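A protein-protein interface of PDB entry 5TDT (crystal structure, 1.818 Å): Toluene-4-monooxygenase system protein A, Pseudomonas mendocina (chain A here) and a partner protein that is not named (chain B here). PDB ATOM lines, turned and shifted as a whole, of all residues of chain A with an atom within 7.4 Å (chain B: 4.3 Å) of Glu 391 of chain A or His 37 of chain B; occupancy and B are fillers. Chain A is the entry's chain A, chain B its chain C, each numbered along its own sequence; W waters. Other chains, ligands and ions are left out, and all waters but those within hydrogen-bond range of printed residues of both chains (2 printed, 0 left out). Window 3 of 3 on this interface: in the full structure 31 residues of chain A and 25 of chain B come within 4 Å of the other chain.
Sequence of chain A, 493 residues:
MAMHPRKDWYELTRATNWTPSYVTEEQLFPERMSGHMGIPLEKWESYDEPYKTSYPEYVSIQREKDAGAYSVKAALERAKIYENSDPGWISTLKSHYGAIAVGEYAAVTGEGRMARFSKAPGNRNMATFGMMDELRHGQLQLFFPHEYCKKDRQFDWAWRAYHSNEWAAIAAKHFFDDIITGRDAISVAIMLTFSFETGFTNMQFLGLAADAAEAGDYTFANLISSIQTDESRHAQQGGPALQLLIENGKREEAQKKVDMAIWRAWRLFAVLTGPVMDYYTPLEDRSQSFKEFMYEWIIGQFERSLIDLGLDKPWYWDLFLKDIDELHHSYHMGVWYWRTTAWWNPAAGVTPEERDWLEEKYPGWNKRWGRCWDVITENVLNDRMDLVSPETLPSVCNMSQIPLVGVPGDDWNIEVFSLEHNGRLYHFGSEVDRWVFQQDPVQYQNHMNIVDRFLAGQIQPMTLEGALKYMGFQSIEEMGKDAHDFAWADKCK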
ATOM      1  N   TYR A 337     -14.979  31.970  18.280  1.00  0.00           N
ATOM      2  CA  TYR A 337     -13.826  31.102  18.522  1.00  0.00           C
ATOM      3  C   TYR A 337     -14.258  29.633  18.653  1.00  0.00           C
ATOM      4  O   TYR A 337     -13.626  28.740  18.076  1.00  0.00           O
ATOM      5  CB  TYR A 337     -13.045  31.586  19.746  1.00  0.00           C
ATOM      6  CG  TYR A 337     -11.607  31.066  19.755  1.00  0.00           C
ATOM      7  CD1 TYR A 337     -11.287  29.885  20.409  1.00  0.00           C
ATOM      8  CD2 TYR A 337     -10.582  31.762  19.094  1.00  0.00           C
ATOM      9  CE1 TYR A 337      -9.979  29.396  20.422  1.00  0.00           C
ATOM     10  CE2 TYR A 337      -9.262  31.278  19.099  1.00  0.00           C
ATOM     11  CZ  TYR A 337      -8.977  30.092  19.766  1.00  0.00           C
ATOM     12  OH  TYR A 337      -7.692  29.598  19.788  1.00  0.00           O
ATOM     13  N   TRP A 338     -15.378  29.372  19.330  1.00  0.00           N
ATOM     14  CA  TRP A 338     -15.949  28.025  19.405  1.00  0.00           C
ATOM     15  C   TRP A 338     -17.012  27.781  18.330  1.00  0.00           C
ATOM     16  O   TRP A 338     -17.991  27.063  18.563  1.00  0.00           O
ATOM     17  CB  TRP A 338     -16.512  27.780  20.809  1.00  0.00           C
ATOM     18  CG  TRP A 338     -15.443  27.369  21.801  1.00  0.00           C
ATOM     19  CD1 TRP A 338     -15.132  26.098  22.200  1.00  0.00           C
ATOM     20  CD2 TRP A 338     -14.543  28.236  22.490  1.00  0.00           C
ATOM     21  NE1 TRP A 338     -14.082  26.119  23.099  1.00  0.00           N
ATOM     22  CE2 TRP A 338     -13.713  27.423  23.303  1.00  0.00           C
ATOM     23  CE3 TRP A 338     -14.371  29.631  22.521  1.00  0.00           C
ATOM     24  CZ2 TRP A 338     -12.718  27.951  24.114  1.00  0.00           C
ATOM     25  CZ3 TRP A 338     -13.373  30.156  23.332  1.00  0.00           C
ATOM     26  CH2 TRP A 338     -12.557  29.314  24.116  1.00  0.00           C
ATOM     27  N   ASP A 386      -4.316  26.313  13.360  1.00  0.00           N
ATOM     28  CA  ASP A 386      -4.562  25.545  14.575  1.00  0.00           C
ATOM     29  C   ASP A 386      -4.753  26.452  15.788  1.00  0.00           C
ATOM     30  O   ASP A 386      -5.395  26.042  16.763  1.00  0.00           O
ATOM     31  CB  ASP A 386      -3.431  24.533  14.814  1.00  0.00           C
ATOM     32  CG  ASP A 386      -2.075  25.192  14.993  1.00  0.00           C
ATOM     33  OD1 ASP A 386      -1.726  26.076  14.180  1.00  0.00           O
ATOM     34  OD2 ASP A 386      -1.359  24.827  15.954  1.00  0.00           O
ATOM     35  N   LEU A 387      -4.242  27.684  15.747  1.00  0.00           N
ATOM     36  CA  LEU A 387      -4.413  28.611  16.859  1.00  0.00           C
ATOM     37  C   LEU A 387      -5.726  29.403  16.793  1.00  0.00           C
ATOM     38  O   LEU A 387      -5.979  30.219  17.682  1.00  0.00           O
ATOM     39  CB  LEU A 387      -3.220  29.578  16.938  1.00  0.00           C
ATOM     40  CG  LEU A 387      -1.811  28.959  17.025  1.00  0.00           C
ATOM     41  CD1 LEU A 387      -0.735  30.026  17.051  1.00  0.00           C
ATOM     42  CD2 LEU A 387      -1.680  28.044  18.233  1.00  0.00           C
ATOM     43  N   SER A 389      -8.681  27.627  16.438  1.00  0.00           N
ATOM     44  CA  SER A 389      -9.664  26.635  16.838  1.00  0.00           C
ATOM     45  C   SER A 389      -9.318  26.154  18.238  1.00  0.00           C
ATOM     46  O   SER A 389      -8.135  25.904  18.528  1.00  0.00           O
ATOM     47  CB  SER A 389      -9.697  25.450  15.863  1.00  0.00           C
ATOM     48  OG  SER A 389     -10.117  25.901  14.585  1.00  0.00           O
ATOM     49  N   PRO A 390     -10.309  26.011  19.120  1.00  0.00           N
ATOM     50  CA  PRO A 390     -10.021  25.668  20.516  1.00  0.00           C
ATOM     51  C   PRO A 390      -9.713  24.187  20.700  1.00  0.00           C
ATOM     52  O   PRO A 390     -10.088  23.329  19.896  1.00  0.00           O
ATOM     53  CB  PRO A 390     -11.318  26.042  21.249  1.00  0.00           C
ATOM     54  CG  PRO A 390     -12.386  25.769  20.218  1.00  0.00           C
ATOM     55  CD  PRO A 390     -11.762  26.149  18.877  1.00  0.00           C
ATOM     56  N   GLU A 391      -9.033  23.910  21.811  1.00  0.00           N
ATOM     57  CA  GLU A 391      -8.678  22.559  22.220  1.00  0.00           C
ATOM     58  C   GLU A 391      -9.121  22.280  23.657  1.00  0.00           C
ATOM     59  O   GLU A 391      -8.676  21.302  24.256  1.00  0.00           O
ATOM     60  CB  GLU A 391      -7.171  22.342  22.055  1.00  0.00           C
ATOM     61  CG  GLU A 391      -6.728  22.315  20.574  1.00  0.00           C
ATOM     62  CD  GLU A 391      -5.208  22.287  20.409  1.00  0.00           C
ATOM     63  OE1 GLU A 391      -4.699  22.848  19.408  1.00  0.00           O
ATOM     64  OE2 GLU A 391      -4.529  21.712  21.283  1.00  0.00           O
ATOM     65  N   THR A 392     -10.001  23.110  24.215  1.00  0.00           N
ATOM     66  CA  THR A 392     -10.609  22.827  25.509  1.00  0.00           C
ATOM     67  C   THR A 392     -12.022  23.403  25.517  1.00  0.00           C
ATOM     68  O   THR A 392     -12.476  23.998  24.535  1.00  0.00           O
ATOM     69  CB  THR A 392      -9.774  23.383  26.669  1.00  0.00           C
ATOM     70  OG1 THR A 392     -10.298  22.882  27.903  1.00  0.00           O
ATOM     71  CG2 THR A 392      -9.826  24.912  26.686  1.00  0.00           C
ATOM     72  N   LEU A 393     -12.750  23.206  26.682  1.00  0.00           N
ATOM     73  CA  LEU A 393     -14.097  23.766  26.822  1.00  0.00           C
ATOM     74  C   LEU A 393     -14.049  25.082  27.588  1.00  0.00           C
ATOM     75  O   LEU A 393     -13.200  25.266  28.465  1.00  0.00           O
ATOM     76  CB  LEU A 393     -15.039  22.795  27.564  1.00  0.00           C
ATOM     77  CG  LEU A 393     -15.245  21.414  26.921  1.00  0.00           C
ATOM     78  CD1 LEU A 393     -16.348  20.594  27.606  1.00  0.00           C
ATOM     79  CD2 LEU A 393     -15.539  21.577  25.448  1.00  0.00           C
ATOM     80  N   LEU A 464     -13.371  16.958  22.975  1.00  0.00           N
ATOM     81  CA  LEU A 464     -14.159  17.963  22.266  1.00  0.00           C
ATOM     82  C   LEU A 464     -14.959  17.340  21.124  1.00  0.00           C
ATOM     83  O   LEU A 464     -16.107  17.727  20.888  1.00  0.00           O
ATOM     84  CB  LEU A 464     -13.261  19.092  21.764  1.00  0.00           C
ATOM     85  CG  LEU A 464     -12.933  20.180  22.793  1.00  0.00           C
ATOM     86  CD1 LEU A 464     -12.206  19.635  24.030  1.00  0.00           C
ATOM     87  CD2 LEU A 464     -12.126  21.287  22.138  1.00  0.00           C
ATOM     88  N   GLN B  17     -11.776  29.239  31.351  1.00  0.00           N
ATOM     89  CA  GLN B  17     -11.731  27.982  30.608  1.00  0.00           C
ATOM     90  C   GLN B  17     -11.458  26.790  31.516  1.00  0.00           C
ATOM     91  O   GLN B  17     -10.705  26.883  32.490  1.00  0.00           O
ATOM     92  CB  GLN B  17     -10.636  28.006  29.519  1.00  0.00           C
ATOM     93  CG  GLN B  17     -10.941  28.875  28.302  1.00  0.00           C
ATOM     94  CD  GLN B  17      -9.783  28.849  27.312  1.00  0.00           C
ATOM     95  OE1 GLN B  17      -8.634  29.137  27.676  1.00  0.00           O
ATOM     96  NE2 GLN B  17     -10.072  28.492  26.074  1.00  0.00           N
ATOM     97  N   LYS B  33       0.266  25.180  31.318  1.00  0.00           N
ATOM     98  CA  LYS B  33      -0.873  24.455  30.767  1.00  0.00           C
ATOM     99  C   LYS B  33      -2.038  25.393  30.463  1.00  0.00           C
ATOM    100  O   LYS B  33      -2.728  25.209  29.455  1.00  0.00           O
ATOM    101  CB  LYS B  33      -1.304  23.341  31.724  1.00  0.00           C
ATOM    102  CG  LYS B  33      -0.389  22.111  31.679  1.00  0.00           C
ATOM    103  CD  LYS B  33      -0.792  21.060  32.729  1.00  0.00           C
ATOM    104  CE  LYS B  33       0.120  19.816  32.660  1.00  0.00           C
ATOM    105  NZ  LYS B  33      -0.252  18.779  33.688  1.00  0.00           N
ATOM    106  N   VAL B  34      -2.272  26.399  31.312  1.00  0.00           N
ATOM    107  CA  VAL B  34      -3.296  27.407  31.016  1.00  0.00           C
ATOM    108  C   VAL B  34      -2.881  28.242  29.812  1.00  0.00           C
ATOM    109  O   VAL B  34      -3.670  28.467  28.886  1.00  0.00           O
ATOM    110  CB  VAL B  34      -3.562  28.310  32.238  1.00  0.00           C
ATOM    111  CG1 VAL B  34      -4.582  29.408  31.888  1.00  0.00           C
ATOM    112  CG2 VAL B  34      -4.047  27.498  33.424  1.00  0.00           C
ATOM    113  N   ALA B  35      -1.631  28.709  29.810  1.00  0.00           N
ATOM    114  CA  ALA B  35      -1.163  29.589  28.747  1.00  0.00           C
ATOM    115  C   ALA B  35      -1.286  28.928  27.390  1.00  0.00           C
ATOM    116  O   ALA B  35      -1.555  29.612  26.393  1.00  0.00           O
ATOM    117  CB  ALA B  35       0.285  30.010  29.008  1.00  0.00           C
ATOM    118  N   TYR B  36      -1.105  27.602  27.338  1.00  0.00           N
ATOM    119  CA  TYR B  36      -1.276  26.861  26.095  1.00  0.00           C
ATOM    120  C   TYR B  36      -2.570  27.245  25.387  1.00  0.00           C
ATOM    121  O   TYR B  36      -2.607  27.337  24.156  1.00  0.00           O
ATOM    122  CB  TYR B  36      -1.264  25.357  26.374  1.00  0.00           C
ATOM    123  CG  TYR B  36      -1.443  24.536  25.119  1.00  0.00           C
ATOM    124  CD1 TYR B  36      -0.339  24.081  24.398  1.00  0.00           C
ATOM    125  CD2 TYR B  36      -2.713  24.228  24.646  1.00  0.00           C
ATOM    126  CE1 TYR B  36      -0.502  23.333  23.232  1.00  0.00           C
ATOM    127  CE2 TYR B  36      -2.887  23.498  23.493  1.00  0.00           C
ATOM    128  CZ  TYR B  36      -1.784  23.042  22.795  1.00  0.00           C
ATOM    129  OH  TYR B  36      -1.981  22.311  21.654  1.00  0.00           O
ATOM    130  N   HIS B  37      -3.638  27.473  26.152  1.00  0.00           N
ATOM    131  CA  HIS B  37      -4.959  27.718  25.597  1.00  0.00           C
ATOM    132  C   HIS B  37      -5.277  29.200  25.440  1.00  0.00           C
ATOM    133  O   HIS B  37      -6.440  29.545  25.186  1.00  0.00           O
ATOM    134  CB  HIS B  37      -6.023  27.048  26.472  1.00  0.00           C
ATOM    135  CG  HIS B  37      -5.877  25.562  26.561  1.00  0.00           C
ATOM    136  ND1 HIS B  37      -6.328  24.708  25.579  1.00  0.00           N
ATOM    137  CD2 HIS B  37      -5.309  24.778  27.509  1.00  0.00           C
ATOM    138  CE1 HIS B  37      -6.062  23.461  25.925  1.00  0.00           C
ATOM    139  NE2 HIS B  37      -5.438  23.476  27.090  1.00  0.00           N
ATOM    140  N   CYS B  38      -4.286  30.081  25.576  1.00  0.00           N
ATOM    141  CA  CYS B  38      -4.562  31.514  25.641  1.00  0.00           C
ATOM    142  C   CYS B  38      -3.526  32.340  24.891  1.00  0.00           C
ATOM    143  O   CYS B  38      -3.877  33.190  24.067  1.00  0.00           O
ATOM    144  CB  CYS B  38      -4.600  31.987  27.099  1.00  0.00           C
ATOM    145  SG  CYS B  38      -5.762  31.106  28.168  1.00  0.00           S
ATOM    146  N   VAL B  39      -2.249  32.147  25.226  1.00  0.00           N
ATOM    147  CA  VAL B  39      -1.185  32.914  24.597  1.00  0.00           C
ATOM    148  C   VAL B  39      -1.057  32.488  23.147  1.00  0.00           C
ATOM    149  O   VAL B  39      -1.127  31.292  22.823  1.00  0.00           O
ATOM    150  CB  VAL B  39       0.139  32.716  25.354  1.00  0.00           C
ATOM    151  CG1 VAL B  39       1.264  33.528  24.702  1.00  0.00           C
ATOM    152  CG2 VAL B  39      -0.040  33.106  26.798  1.00  0.00           C
ATOM    153  N   ARG B  41      -3.247  32.739  21.073  1.00  0.00           N
ATOM    154  CA  ARG B  41      -4.591  32.462  20.587  1.00  0.00           C
ATOM    155  C   ARG B  41      -5.453  33.716  20.637  1.00  0.00           C
ATOM    156  O   ARG B  41      -6.019  34.134  19.622  1.00  0.00           O
ATOM    157  CB  ARG B  41      -5.237  31.323  21.397  1.00  0.00           C
ATOM    158  CG  ARG B  41      -4.605  29.959  21.096  1.00  0.00           C
ATOM    159  CD  ARG B  41      -5.126  28.838  22.000  1.00  0.00           C
ATOM    160  NE  ARG B  41      -4.406  27.598  21.715  1.00  0.00           N
ATOM    161  CZ  ARG B  41      -4.749  26.744  20.753  1.00  0.00           C
ATOM    162  NH1 ARG B  41      -5.808  26.990  19.986  1.00  0.00           N
ATOM    163  NH2 ARG B  41      -4.031  25.647  20.548  1.00  0.00           N
ATOM    164  N   ARG B  42      -5.550  34.332  21.806  1.00  0.00           N
ATOM    165  CA  ARG B  42      -6.275  35.576  21.986  1.00  0.00           C
ATOM    166  C   ARG B  42      -5.478  36.565  22.828  1.00  0.00           C
ATOM    167  O   ARG B  42      -5.938  37.692  23.047  1.00  0.00           O
ATOM    168  CB  ARG B  42      -7.638  35.294  22.635  1.00  0.00           C
ATOM    169  CG  ARG B  42      -8.549  34.349  21.827  1.00  0.00           C
ATOM    170  CD  ARG B  42      -9.801  33.933  22.629  1.00  0.00           C
ATOM    171  NE  ARG B  42      -9.403  33.313  23.888  1.00  0.00           N
ATOM    172  CZ  ARG B  42      -9.054  32.033  24.029  1.00  0.00           C
ATOM    173  NH1 ARG B  42      -8.656  31.586  25.215  1.00  0.00           N
ATOM    174  NH2 ARG B  42      -9.093  31.200  22.995  1.00  0.00           N
HETATM  175  O   HOH W   1      -7.497  25.932  23.102  1.00  0.00           O
HETATM  176  O   HOH W   2      -5.932  33.096  17.157  1.00  0.00           O
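Printed residues of chain B within 4 Å of Trp 338 of chain A: Gln 17 (3.3 Å).
Of the printed residues of chain B, Leu 387 of chain A touches Arg 41.
Pro 390 of chain A touches none of the printed residues of chain B.
Of chain B, only Tyr 36 (2.6 Å), His 37 (3.8 Å) and Arg 41 (3.1 Å) come within 4 Å of Glu 391 of chain A.
Printed residues of chain A within 4 Å of Gln 17 of chain B: Trp 338, Thr 392 and Leu 393.
Lys 33 of chain B touches none of the printed residues of chain A.
Printed residues of chain A within 4 Å of Arg 42 of chain B: Tyr 337.
The nearest printed residue of chain B that does not touch Leu 393 of chain A is His 37 of chain B (6.7 Å).
The side-chain hydroxyl (OH) of Tyr 337 of chain A lies within hydrogen-bond range of the backbone carbonyl oxygen (O) of Leu 387 of chain A (2.8 Å).
The indole nitrogen of Trp 338 of chain A is in hydrogen-bond range of the backbone carbonyl oxygen of Thr 392 of chain A, 3.0 Å away.
The side-chain amide oxygen of Gln 17 of chain B sits close to the backbone carbonyl oxygen of His 37 of chain B, at 3.3 Å.
SG of Cys 38 of chain B is in hydrogen-bond range of OE1 of Gln 17 of chain B (3.5 Å).
The guanidinium group of Arg 41 of chain B lies within hydrogen-bond range of the backbone carbonyl oxygen of Tyr 36 of chain B, 3.0 Å away.
The guanidinium group of Arg 42 of chain B sits at hydrogen-bond distance from the backbone carbonyl oxygen of His 37 of chain B (3.0 Å).
Of the 10 printed residues of chain A, 8 touch a printed residue of chain B.
Along chain A the printed residues that touch a printed residue of chain B span positions 337 to 393.
Printed residues of chain B that touch a printed residue of chain A: Gln 17, Tyr 36, His 37, Arg 41 and Arg 42.
Hydrophobic or aromatic side chains of chain B within 4 Å of the printed part of chain A: Tyr 36 and His 37.
Along chain B the printed residues that touch a printed residue of chain A span positions 17 to 42.
Among the printed residues, merely in contact across the chains: Tyr 337 of chain A with Arg 42 of chain B, Trp 338 of chain A with Gln 17 of chain B, Thr 392 of chain A with Gln 17 of chain B, Thr 392 of chain A with His 37 of chain B, Leu 387 of chain A with Arg 41 of chain B, Leu 393 of chain A with Gln 17 of chain B and Glu 391 of chain A with His 37 of chain B.
OH of Tyr 337 of chain A lies within hydrogen-bond range of NH1 of Arg 41 of chain B (3.2 Å).
The backbone carbonyl oxygen (O) of Asp 386 of chain A sits at hydrogen-bond distance from the guanidinium group (NH1) of Arg 41 of chain B (3.4 Å).
The backbone carbonyl oxygen (O) of Ser 389 of chain A is in hydrogen-bond range of the guanidinium group (NH1) of Arg 41 of chain B (3.0 Å).
OH of Tyr 36 of chain B lies within hydrogen-bond range of OE2 of Glu 391 of chain A, 2.6 Å away.
OE1 of Glu 391 of chain A lies within salt-bridge range of NH2 of Arg 41 of chain B (3.1 Å).
Water W2 lies within hydrogen-bond range of the backbone carbonyl oxygen (O) of Arg 41 of chain B (2.7 Å) and the backbone carbonyl oxygen (O) of Leu 387 of chain A (2.9 Å).
Water W1 bridges the backbone NH of Glu 391 of chain A (2.8 Å) and a ring nitrogen (ND1) of His 37 of chain B (3.0 Å).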
